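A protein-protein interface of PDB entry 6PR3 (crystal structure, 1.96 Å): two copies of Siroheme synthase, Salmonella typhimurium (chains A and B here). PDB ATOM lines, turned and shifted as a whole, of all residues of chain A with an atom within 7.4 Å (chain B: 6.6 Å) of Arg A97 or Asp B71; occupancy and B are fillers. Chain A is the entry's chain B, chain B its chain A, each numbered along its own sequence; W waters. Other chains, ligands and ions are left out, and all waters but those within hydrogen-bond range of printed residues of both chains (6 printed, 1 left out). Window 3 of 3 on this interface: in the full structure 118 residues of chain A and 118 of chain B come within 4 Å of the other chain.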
ATOM      1  N   CYS A  73       4.272  18.450  17.207  1.00  0.00           N
ATOM      2  CA  CYS A  73       5.217  17.431  17.660  1.00  0.00           C
ATOM      3  C   CYS A  73       4.547  16.083  17.901  1.00  0.00           C
ATOM      4  O   CYS A  73       3.401  16.006  18.355  1.00  0.00           O
ATOM      5  CB  CYS A  73       5.926  17.873  18.940  1.00  0.00           C
ATOM      6  SG  CYS A  73       7.252  19.030  18.616  1.00  0.00           S
ATOM      7  N   TRP A  74       5.299  15.023  17.615  1.00  0.00           N
ATOM      8  CA  TRP A  74       4.907  13.636  17.838  1.00  0.00           C
ATOM      9  C   TRP A  74       5.419  13.050  19.143  1.00  0.00           C
ATOM     10  O   TRP A  74       4.811  12.108  19.666  1.00  0.00           O
ATOM     11  CB  TRP A  74       5.420  12.760  16.697  1.00  0.00           C
ATOM     12  CG  TRP A  74       4.776  13.080  15.346  1.00  0.00           C
ATOM     13  CD1 TRP A  74       5.006  14.185  14.564  1.00  0.00           C
ATOM     14  CD2 TRP A  74       3.840  12.273  14.632  1.00  0.00           C
ATOM     15  NE1 TRP A  74       4.271  14.109  13.415  1.00  0.00           N
ATOM     16  CE2 TRP A  74       3.544  12.946  13.425  1.00  0.00           C
ATOM     17  CE3 TRP A  74       3.227  11.036  14.888  1.00  0.00           C
ATOM     18  CZ2 TRP A  74       2.655  12.427  12.472  1.00  0.00           C
ATOM     19  CZ3 TRP A  74       2.347  10.525  13.943  1.00  0.00           C
ATOM     20  CH2 TRP A  74       2.070  11.218  12.751  1.00  0.00           C
ATOM     21  N   ASP A  91       2.612  18.409  31.362  1.00  0.00           N
ATOM     22  CA  ASP A  91       1.213  18.837  31.313  1.00  0.00           C
ATOM     23  C   ASP A  91       0.835  19.328  29.924  1.00  0.00           C
ATOM     24  O   ASP A  91      -0.262  19.032  29.431  1.00  0.00           O
ATOM     25  CB  ASP A  91       0.935  19.935  32.347  1.00  0.00           C
ATOM     26  CG  ASP A  91       0.965  19.415  33.780  1.00  0.00           C
ATOM     27  OD1 ASP A  91       0.793  18.196  33.972  1.00  0.00           O
ATOM     28  OD2 ASP A  91       1.155  20.226  34.711  1.00  0.00           O
ATOM     29  N   ALA A  92       1.727  20.085  29.273  1.00  0.00           N
ATOM     30  CA  ALA A  92       1.417  20.624  27.953  1.00  0.00           C
ATOM     31  C   ALA A  92       1.331  19.515  26.905  1.00  0.00           C
ATOM     32  O   ALA A  92       0.486  19.573  26.002  1.00  0.00           O
ATOM     33  CB  ALA A  92       2.472  21.658  27.553  1.00  0.00           C
ATOM     34  N   ALA A  93       2.211  18.510  26.998  1.00  0.00           N
ATOM     35  CA  ALA A  93       2.143  17.349  26.104  1.00  0.00           C
ATOM     36  C   ALA A  93       0.858  16.559  26.316  1.00  0.00           C
ATOM     37  O   ALA A  93       0.183  16.166  25.354  1.00  0.00           O
ATOM     38  CB  ALA A  93       3.367  16.438  26.331  1.00  0.00           C
ATOM     39  N   GLU A  94       0.487  16.342  27.574  1.00  0.00           N
ATOM     40  CA  GLU A  94      -0.698  15.547  27.881  1.00  0.00           C
ATOM     41  C   GLU A  94      -1.961  16.168  27.291  1.00  0.00           C
ATOM     42  O   GLU A  94      -2.823  15.458  26.756  1.00  0.00           O
ATOM     43  CB  GLU A  94      -0.818  15.399  29.397  1.00  0.00           C
ATOM     44  CG  GLU A  94      -2.171  14.927  29.879  1.00  0.00           C
ATOM     45  CD  GLU A  94      -2.332  13.444  29.693  1.00  0.00           C
ATOM     46  OE1 GLU A  94      -3.479  12.952  29.761  1.00  0.00           O
ATOM     47  OE2 GLU A  94      -1.298  12.773  29.484  1.00  0.00           O
ATOM     48  N   SER A  95      -2.095  17.492  27.384  1.00  0.00           N
ATOM     49  CA  SER A  95      -3.277  18.143  26.810  1.00  0.00           C
ATOM     50  C   SER A  95      -3.315  18.049  25.281  1.00  0.00           C
ATOM     51  O   SER A  95      -4.398  18.147  24.691  1.00  0.00           O
ATOM     52  CB  SER A  95      -3.340  19.609  27.263  1.00  0.00           C
ATOM     53  OG  SER A  95      -2.237  20.348  26.762  1.00  0.00           O
ATOM     54  N   ARG A  96      -2.171  17.855  24.620  1.00  0.00           N
ATOM     55  CA  ARG A  96      -2.133  17.699  23.167  1.00  0.00           C
ATOM     56  C   ARG A  96      -2.051  16.243  22.721  1.00  0.00           C
ATOM     57  O   ARG A  96      -1.920  15.983  21.514  1.00  0.00           O
ATOM     58  CB  ARG A  96      -0.952  18.479  22.579  1.00  0.00           C
ATOM     59  CG  ARG A  96      -1.055  20.014  22.720  1.00  0.00           C
ATOM     60  CD  ARG A  96       0.321  20.664  22.467  1.00  0.00           C
ATOM     61  NE  ARG A  96       0.200  22.114  22.291  1.00  0.00           N
ATOM     62  CZ  ARG A  96       0.035  22.965  23.294  1.00  0.00           C
ATOM     63  NH1 ARG A  96      -0.020  22.510  24.549  1.00  0.00           N
ATOM     64  NH2 ARG A  96      -0.072  24.267  23.053  1.00  0.00           N
ATOM     65  N   ARG A  97      -2.093  15.296  23.659  1.00  0.00           N
ATOM     66  CA  ARG A  97      -2.002  13.866  23.360  1.00  0.00           C
ATOM     67  C   ARG A  97      -0.681  13.539  22.655  1.00  0.00           C
ATOM     68  O   ARG A  97      -0.628  12.757  21.702  1.00  0.00           O
ATOM     69  CB  ARG A  97      -3.222  13.405  22.546  1.00  0.00           C
ATOM     70  CG  ARG A  97      -4.550  13.619  23.318  1.00  0.00           C
ATOM     71  CD  ARG A  97      -5.825  13.496  22.479  1.00  0.00           C
ATOM     72  NE  ARG A  97      -5.760  14.309  21.266  1.00  0.00           N
ATOM     73  CZ  ARG A  97      -6.143  15.578  21.186  1.00  0.00           C
ATOM     74  NH1 ARG A  97      -6.633  16.203  22.256  1.00  0.00           N
ATOM     75  NH2 ARG A  97      -6.026  16.221  20.031  1.00  0.00           N
ATOM     76  N   ILE A  98       0.399  14.161  23.121  1.00  0.00           N
ATOM     77  CA  ILE A  98       1.758  13.868  22.664  1.00  0.00           C
ATOM     78  C   ILE A  98       2.438  12.992  23.711  1.00  0.00           C
ATOM     79  O   ILE A  98       2.576  13.395  24.872  1.00  0.00           O
ATOM     80  CB  ILE A  98       2.552  15.163  22.431  1.00  0.00           C
ATOM     81  CG1 ILE A  98       1.858  16.011  21.358  1.00  0.00           C
ATOM     82  CG2 ILE A  98       3.994  14.849  22.073  1.00  0.00           C
ATOM     83  CD1 ILE A  98       2.381  17.458  21.308  1.00  0.00           C
ATOM     84  N   PHE A  99       2.873  11.799  23.308  1.00  0.00           N
ATOM     85  CA  PHE A  99       3.611  10.945  24.222  1.00  0.00           C
ATOM     86  C   PHE A  99       4.838  11.676  24.735  1.00  0.00           C
ATOM     87  O   PHE A  99       5.593  12.285  23.966  1.00  0.00           O
ATOM     88  CB  PHE A  99       3.982   9.624  23.538  1.00  0.00           C
ATOM     89  CG  PHE A  99       2.851   8.626  23.535  1.00  0.00           C
ATOM     90  CD1 PHE A  99       2.240   8.250  22.351  1.00  0.00           C
ATOM     91  CD2 PHE A  99       2.368   8.096  24.737  1.00  0.00           C
ATOM     92  CE1 PHE A  99       1.200   7.352  22.354  1.00  0.00           C
ATOM     93  CE2 PHE A  99       1.318   7.206  24.743  1.00  0.00           C
ATOM     94  CZ  PHE A  99       0.723   6.832  23.541  1.00  0.00           C
ATOM     95  N   CYS A 100       4.996  11.670  26.052  1.00  0.00           N
ATOM     96  CA  CYS A 100       6.005  12.487  26.702  1.00  0.00           C
ATOM     97  C   CYS A 100       6.751  11.666  27.745  1.00  0.00           C
ATOM     98  O   CYS A 100       6.143  10.882  28.479  1.00  0.00           O
ATOM     99  CB  CYS A 100       5.354  13.714  27.369  1.00  0.00           C
ATOM    100  SG  CYS A 100       6.560  14.786  28.208  1.00  0.00           S
ATOM    101  N   SER A 110       4.025   9.894  29.938  1.00  0.00           N
ATOM    102  CA  SER A 110       3.236   8.900  29.216  1.00  0.00           C
ATOM    103  C   SER A 110       4.055   7.843  28.470  1.00  0.00           C
ATOM    104  O   SER A 110       3.449   6.910  27.922  1.00  0.00           O
ATOM    105  CB  SER A 110       2.277   9.595  28.232  1.00  0.00           C
ATOM    106  OG  SER A 110       2.944  10.598  27.488  1.00  0.00           O
ATOM    107  N   ASP B  14      -7.415   7.054  25.142  1.00  0.00           N
ATOM    108  CA  ASP B  14      -8.233   6.568  24.037  1.00  0.00           C
ATOM    109  C   ASP B  14      -7.358   6.028  22.919  1.00  0.00           C
ATOM    110  O   ASP B  14      -6.416   6.694  22.484  1.00  0.00           O
ATOM    111  CB  ASP B  14      -9.107   7.683  23.462  1.00  0.00           C
ATOM    112  CG  ASP B  14     -10.015   8.315  24.492  1.00  0.00           C
ATOM    113  OD1 ASP B  14     -10.082   7.803  25.628  1.00  0.00           O
ATOM    114  OD2 ASP B  14     -10.681   9.310  24.145  1.00  0.00           O
ATOM    115  N   GLU B  67     -13.709   8.814  10.567  1.00  0.00           N
ATOM    116  CA  GLU B  67     -12.483   9.550  10.850  1.00  0.00           C
ATOM    117  C   GLU B  67     -12.557  10.284  12.186  1.00  0.00           C
ATOM    118  O   GLU B  67     -11.542  10.430  12.872  1.00  0.00           O
ATOM    119  CB  GLU B  67     -12.219  10.578   9.738  1.00  0.00           C
ATOM    120  CG  GLU B  67     -11.777   9.986   8.414  1.00  0.00           C
ATOM    121  CD  GLU B  67     -12.929   9.623   7.479  1.00  0.00           C
ATOM    122  OE1 GLU B  67     -12.663   9.533   6.261  1.00  0.00           O
ATOM    123  OE2 GLU B  67     -14.083   9.428   7.944  1.00  0.00           O
ATOM    124  N   THR B  68     -13.732  10.806  12.544  1.00  0.00           N
ATOM    125  CA  THR B  68     -13.790  11.583  13.778  1.00  0.00           C
ATOM    126  C   THR B  68     -13.535  10.728  15.009  1.00  0.00           C
ATOM    127  O   THR B  68     -13.269  11.279  16.081  1.00  0.00           O
ATOM    128  CB  THR B  68     -15.126  12.313  13.908  1.00  0.00           C
ATOM    129  OG1 THR B  68     -16.171  11.381  14.228  1.00  0.00           O
ATOM    130  CG2 THR B  68     -15.490  13.065  12.592  1.00  0.00           C
ATOM    131  N   LEU B  69     -13.589   9.399  14.897  1.00  0.00           N
ATOM    132  CA  LEU B  69     -13.271   8.591  16.068  1.00  0.00           C
ATOM    133  C   LEU B  69     -11.806   8.713  16.467  1.00  0.00           C
ATOM    134  O   LEU B  69     -11.439   8.329  17.590  1.00  0.00           O
ATOM    135  CB  LEU B  69     -13.620   7.126  15.812  1.00  0.00           C
ATOM    136  CG  LEU B  69     -15.111   6.814  15.734  1.00  0.00           C
ATOM    137  CD1 LEU B  69     -15.271   5.341  15.434  1.00  0.00           C
ATOM    138  CD2 LEU B  69     -15.827   7.185  17.032  1.00  0.00           C
ATOM    139  N   LEU B  70     -10.957   9.226  15.579  1.00  0.00           N
ATOM    140  CA  LEU B  70      -9.568   9.462  15.964  1.00  0.00           C
ATOM    141  C   LEU B  70      -9.393  10.715  16.810  1.00  0.00           C
ATOM    142  O   LEU B  70      -8.288  10.958  17.309  1.00  0.00           O
ATOM    143  CB  LEU B  70      -8.676   9.594  14.727  1.00  0.00           C
ATOM    144  CG  LEU B  70      -8.501   8.255  13.982  1.00  0.00           C
ATOM    145  CD1 LEU B  70      -8.033   8.532  12.598  1.00  0.00           C
ATOM    146  CD2 LEU B  70      -7.502   7.348  14.678  1.00  0.00           C
ATOM    147  N   ASP B  71     -10.436  11.516  16.999  1.00  0.00           N
ATOM    148  CA  ASP B  71     -10.184  12.868  17.484  1.00  0.00           C
ATOM    149  C   ASP B  71      -9.540  12.889  18.863  1.00  0.00           C
ATOM    150  O   ASP B  71      -8.678  13.734  19.136  1.00  0.00           O
ATOM    151  CB  ASP B  71     -11.471  13.674  17.455  1.00  0.00           C
ATOM    152  CG  ASP B  71     -11.807  14.087  16.037  1.00  0.00           C
ATOM    153  OD1 ASP B  71     -10.965  13.751  15.162  1.00  0.00           O
ATOM    154  OD2 ASP B  71     -12.880  14.662  15.795  1.00  0.00           O
ATOM    155  N   SER B  72      -9.907  11.973  19.745  1.00  0.00           N
ATOM    156  CA  SER B  72      -9.266  12.012  21.059  1.00  0.00           C
ATOM    157  C   SER B  72      -8.154  10.974  21.241  1.00  0.00           C
ATOM    158  O   SER B  72      -7.710  10.756  22.372  1.00  0.00           O
ATOM    159  CB  SER B  72     -10.316  11.848  22.154  1.00  0.00           C
ATOM    160  OG  SER B  72     -10.851  10.531  22.122  1.00  0.00           O
ATOM    161  N   CYS B  73      -7.651  10.372  20.172  1.00  0.00           N
ATOM    162  CA  CYS B  73      -6.844   9.168  20.322  1.00  0.00           C
ATOM    163  C   CYS B  73      -5.350   9.447  20.444  1.00  0.00           C
ATOM    164  O   CYS B  73      -4.838  10.460  19.961  1.00  0.00           O
ATOM    165  CB  CYS B  73      -7.082   8.216  19.150  1.00  0.00           C
ATOM    166  SG  CYS B  73      -8.652   7.356  19.366  1.00  0.00           S
ATOM    167  N   TRP B  74      -4.662   8.518  21.118  1.00  0.00           N
ATOM    168  CA  TRP B  74      -3.210   8.486  21.238  1.00  0.00           C
ATOM    169  C   TRP B  74      -2.555   7.467  20.315  1.00  0.00           C
ATOM    170  O   TRP B  74      -1.388   7.647  19.942  1.00  0.00           O
ATOM    171  CB  TRP B  74      -2.809   8.151  22.677  1.00  0.00           C
ATOM    172  CG  TRP B  74      -3.226   9.173  23.730  1.00  0.00           C
ATOM    173  CD1 TRP B  74      -4.490   9.442  24.159  1.00  0.00           C
ATOM    174  CD2 TRP B  74      -2.351  10.021  24.496  1.00  0.00           C
ATOM    175  NE1 TRP B  74      -4.460  10.406  25.143  1.00  0.00           N
ATOM    176  CE2 TRP B  74      -3.157  10.771  25.372  1.00  0.00           C
ATOM    177  CE3 TRP B  74      -0.962  10.217  24.522  1.00  0.00           C
ATOM    178  CZ2 TRP B  74      -2.627  11.717  26.266  1.00  0.00           C
ATOM    179  CZ3 TRP B  74      -0.433  11.154  25.419  1.00  0.00           C
ATOM    180  CH2 TRP B  74      -1.271  11.894  26.270  1.00  0.00           C
ATOM    181  N   ARG B  96      -3.506  14.024  12.227  1.00  0.00           N
ATOM    182  CA  ARG B  96      -3.687  14.332  13.645  1.00  0.00           C
ATOM    183  C   ARG B  96      -2.434  14.053  14.492  1.00  0.00           C
ATOM    184  O   ARG B  96      -2.486  14.202  15.721  1.00  0.00           O
ATOM    185  CB  ARG B  96      -4.859  13.509  14.212  1.00  0.00           C
ATOM    186  CG  ARG B  96      -6.219  13.817  13.607  1.00  0.00           C
ATOM    187  CD  ARG B  96      -7.259  12.758  13.957  1.00  0.00           C
ATOM    188  NE  ARG B  96      -8.609  13.195  13.593  1.00  0.00           N
ATOM    189  CZ  ARG B  96      -9.081  13.277  12.346  1.00  0.00           C
ATOM    190  NH1 ARG B  96      -8.326  12.960  11.297  1.00  0.00           N
ATOM    191  NH2 ARG B  96     -10.323  13.701  12.141  1.00  0.00           N
ATOM    192  N   ARG B  97      -1.332  13.631  13.863  1.00  0.00           N
ATOM    193  CA  ARG B  97      -0.088  13.263  14.549  1.00  0.00           C
ATOM    194  C   ARG B  97      -0.353  12.176  15.588  1.00  0.00           C
ATOM    195  O   ARG B  97       0.106  12.239  16.728  1.00  0.00           O
ATOM    196  CB  ARG B  97       0.600  14.487  15.167  1.00  0.00           C
ATOM    197  CG  ARG B  97       0.970  15.552  14.109  1.00  0.00           C
ATOM    198  CD  ARG B  97       1.360  16.876  14.709  1.00  0.00           C
ATOM    199  NE  ARG B  97       0.330  17.411  15.599  1.00  0.00           N
ATOM    200  CZ  ARG B  97      -0.745  18.071  15.190  1.00  0.00           C
ATOM    201  NH1 ARG B  97      -0.946  18.289  13.892  1.00  0.00           N
ATOM    202  NH2 ARG B  97      -1.624  18.510  16.081  1.00  0.00           N
ATOM    203  N   ILE B  98      -1.117  11.170  15.174  1.00  0.00           N
ATOM    204  CA  ILE B  98      -1.400  10.000  15.991  1.00  0.00           C
ATOM    205  C   ILE B  98      -0.589   8.853  15.420  1.00  0.00           C
ATOM    206  O   ILE B  98      -0.743   8.520  14.235  1.00  0.00           O
ATOM    207  CB  ILE B  98      -2.902   9.666  15.991  1.00  0.00           C
ATOM    208  CG1 ILE B  98      -3.702  10.816  16.597  1.00  0.00           C
ATOM    209  CG2 ILE B  98      -3.171   8.316  16.746  1.00  0.00           C
ATOM    210  CD1 ILE B  98      -5.241  10.682  16.308  1.00  0.00           C
HETATM  211  O   HOH W   1       1.194  13.685  18.813  1.00  0.00           O
HETATM  212  O   HOH W   2      -4.210  15.790  17.236  1.00  0.00           O
HETATM  213  O   HOH W   3      -6.936  14.325  17.303  1.00  0.00           O
HETATM  214  O   HOH W   4       0.617  17.044  18.087  1.00  0.00           O
HETATM  215  O   HOH W   5      -4.944  13.082  19.078  1.00  0.00           O
HETATM  216  O   HOH W   6      -2.583  17.858  19.380  1.00  0.00           O
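Of chain B, only Asp B71 (3.7 Å), Ser B72 (3.3 Å) and Trp B74 (3.6 Å) come within 4 Å of Arg A97. Printed residues of chain B within 4 Å of Phe A99: Trp B74. Of chain A, only Arg A97 comes within 4 Å of Asp B71. Of the printed residues of chain A, Ile B98 touches Trp A74 (3.7 Å). The nearest residue of chain B that does not touch Arg A97 is Cys B73 (4.1 Å). The nearest printed residue of chain A that does not touch Ser B72 is Arg A96 (7.8 Å).
Trp A74 touches Arg B97, and with the chains exchanged Arg A97 touches Trp B74. Trp A74 touches Ile B98, and with the chains exchanged Ile A98 touches Trp B74. Of the 9 pairs that touch across the chains among the printed residues, 4 have their exchanged pair printed and touching as well.
Among the printed residues, pairs that only touch across the chains: Trp A74 with Arg B97, Trp A74 with Ile B98, Glu A94 with Trp B74, Arg A97 with Asp B71, Arg A97 with Ser B72, Arg A97 with Trp B74, Ile A98 with Trp B74, Phe A99 with Trp B74 and Ser A110 with Trp B74.
O of Asp B14 is in hydrogen-bond range of N of Trp B74, at 2.9 Å. The side-chain carboxylate (OD1) of Asp B71 lies within salt-bridge range of the guanidinium group (NE) of Arg B96 (2.9 Å). The backbone NH (N) of Ile A98 lies within hydrogen-bond range of the backbone carbonyl oxygen (O) of Ala A93, at 3.0 Å. The side-chain hydroxyl (OG) of Ser A110 lies within hydrogen-bond range of the backbone NH (N) of Cys A100, 2.7 Å away.
Of the 13 printed residues of chain A, 6 touch a printed residue of chain B. Hydrophobic or aromatic side chains of chain A within 4 Å of the printed part of chain B: Trp A74 and Phe A99. Hydrophobic or aromatic side chains of chain B that line the printed part of chain A: Trp B74. Among the printed residues, no Asp or Glu carboxylate lies within 4 Å of a Lys or Arg side-chain nitrogen of the other chain.
Water W4 lies within hydrogen-bond range of the guanidinium group (NE) of Arg B97 (2.5 Å) and the backbone carbonyl oxygen (O) of Cys A73 (3.0 Å). Water W3 bridges the backbone carbonyl oxygen of Asp B71 (2.6 Å) and the guanidinium group of Arg A97 (3.4 Å). Water W5 bridges the guanidinium group (NE) of Arg A97 and the backbone carbonyl oxygen (O) of Cys B73. Water W1 bridges the backbone carbonyl oxygen of Arg B97 (2.8 Å) and the backbone carbonyl oxygen of Cys A73 (3.2 Å). Water W2 bridges the backbone carbonyl oxygen (O) of Arg B96 (2.8 Å) and the guanidinium group (NH2) of Arg A97 (3.4 Å). Water W6 bridges O of Arg A96 (2.9 Å) and NH2 of Arg B97 (3.5 Å).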
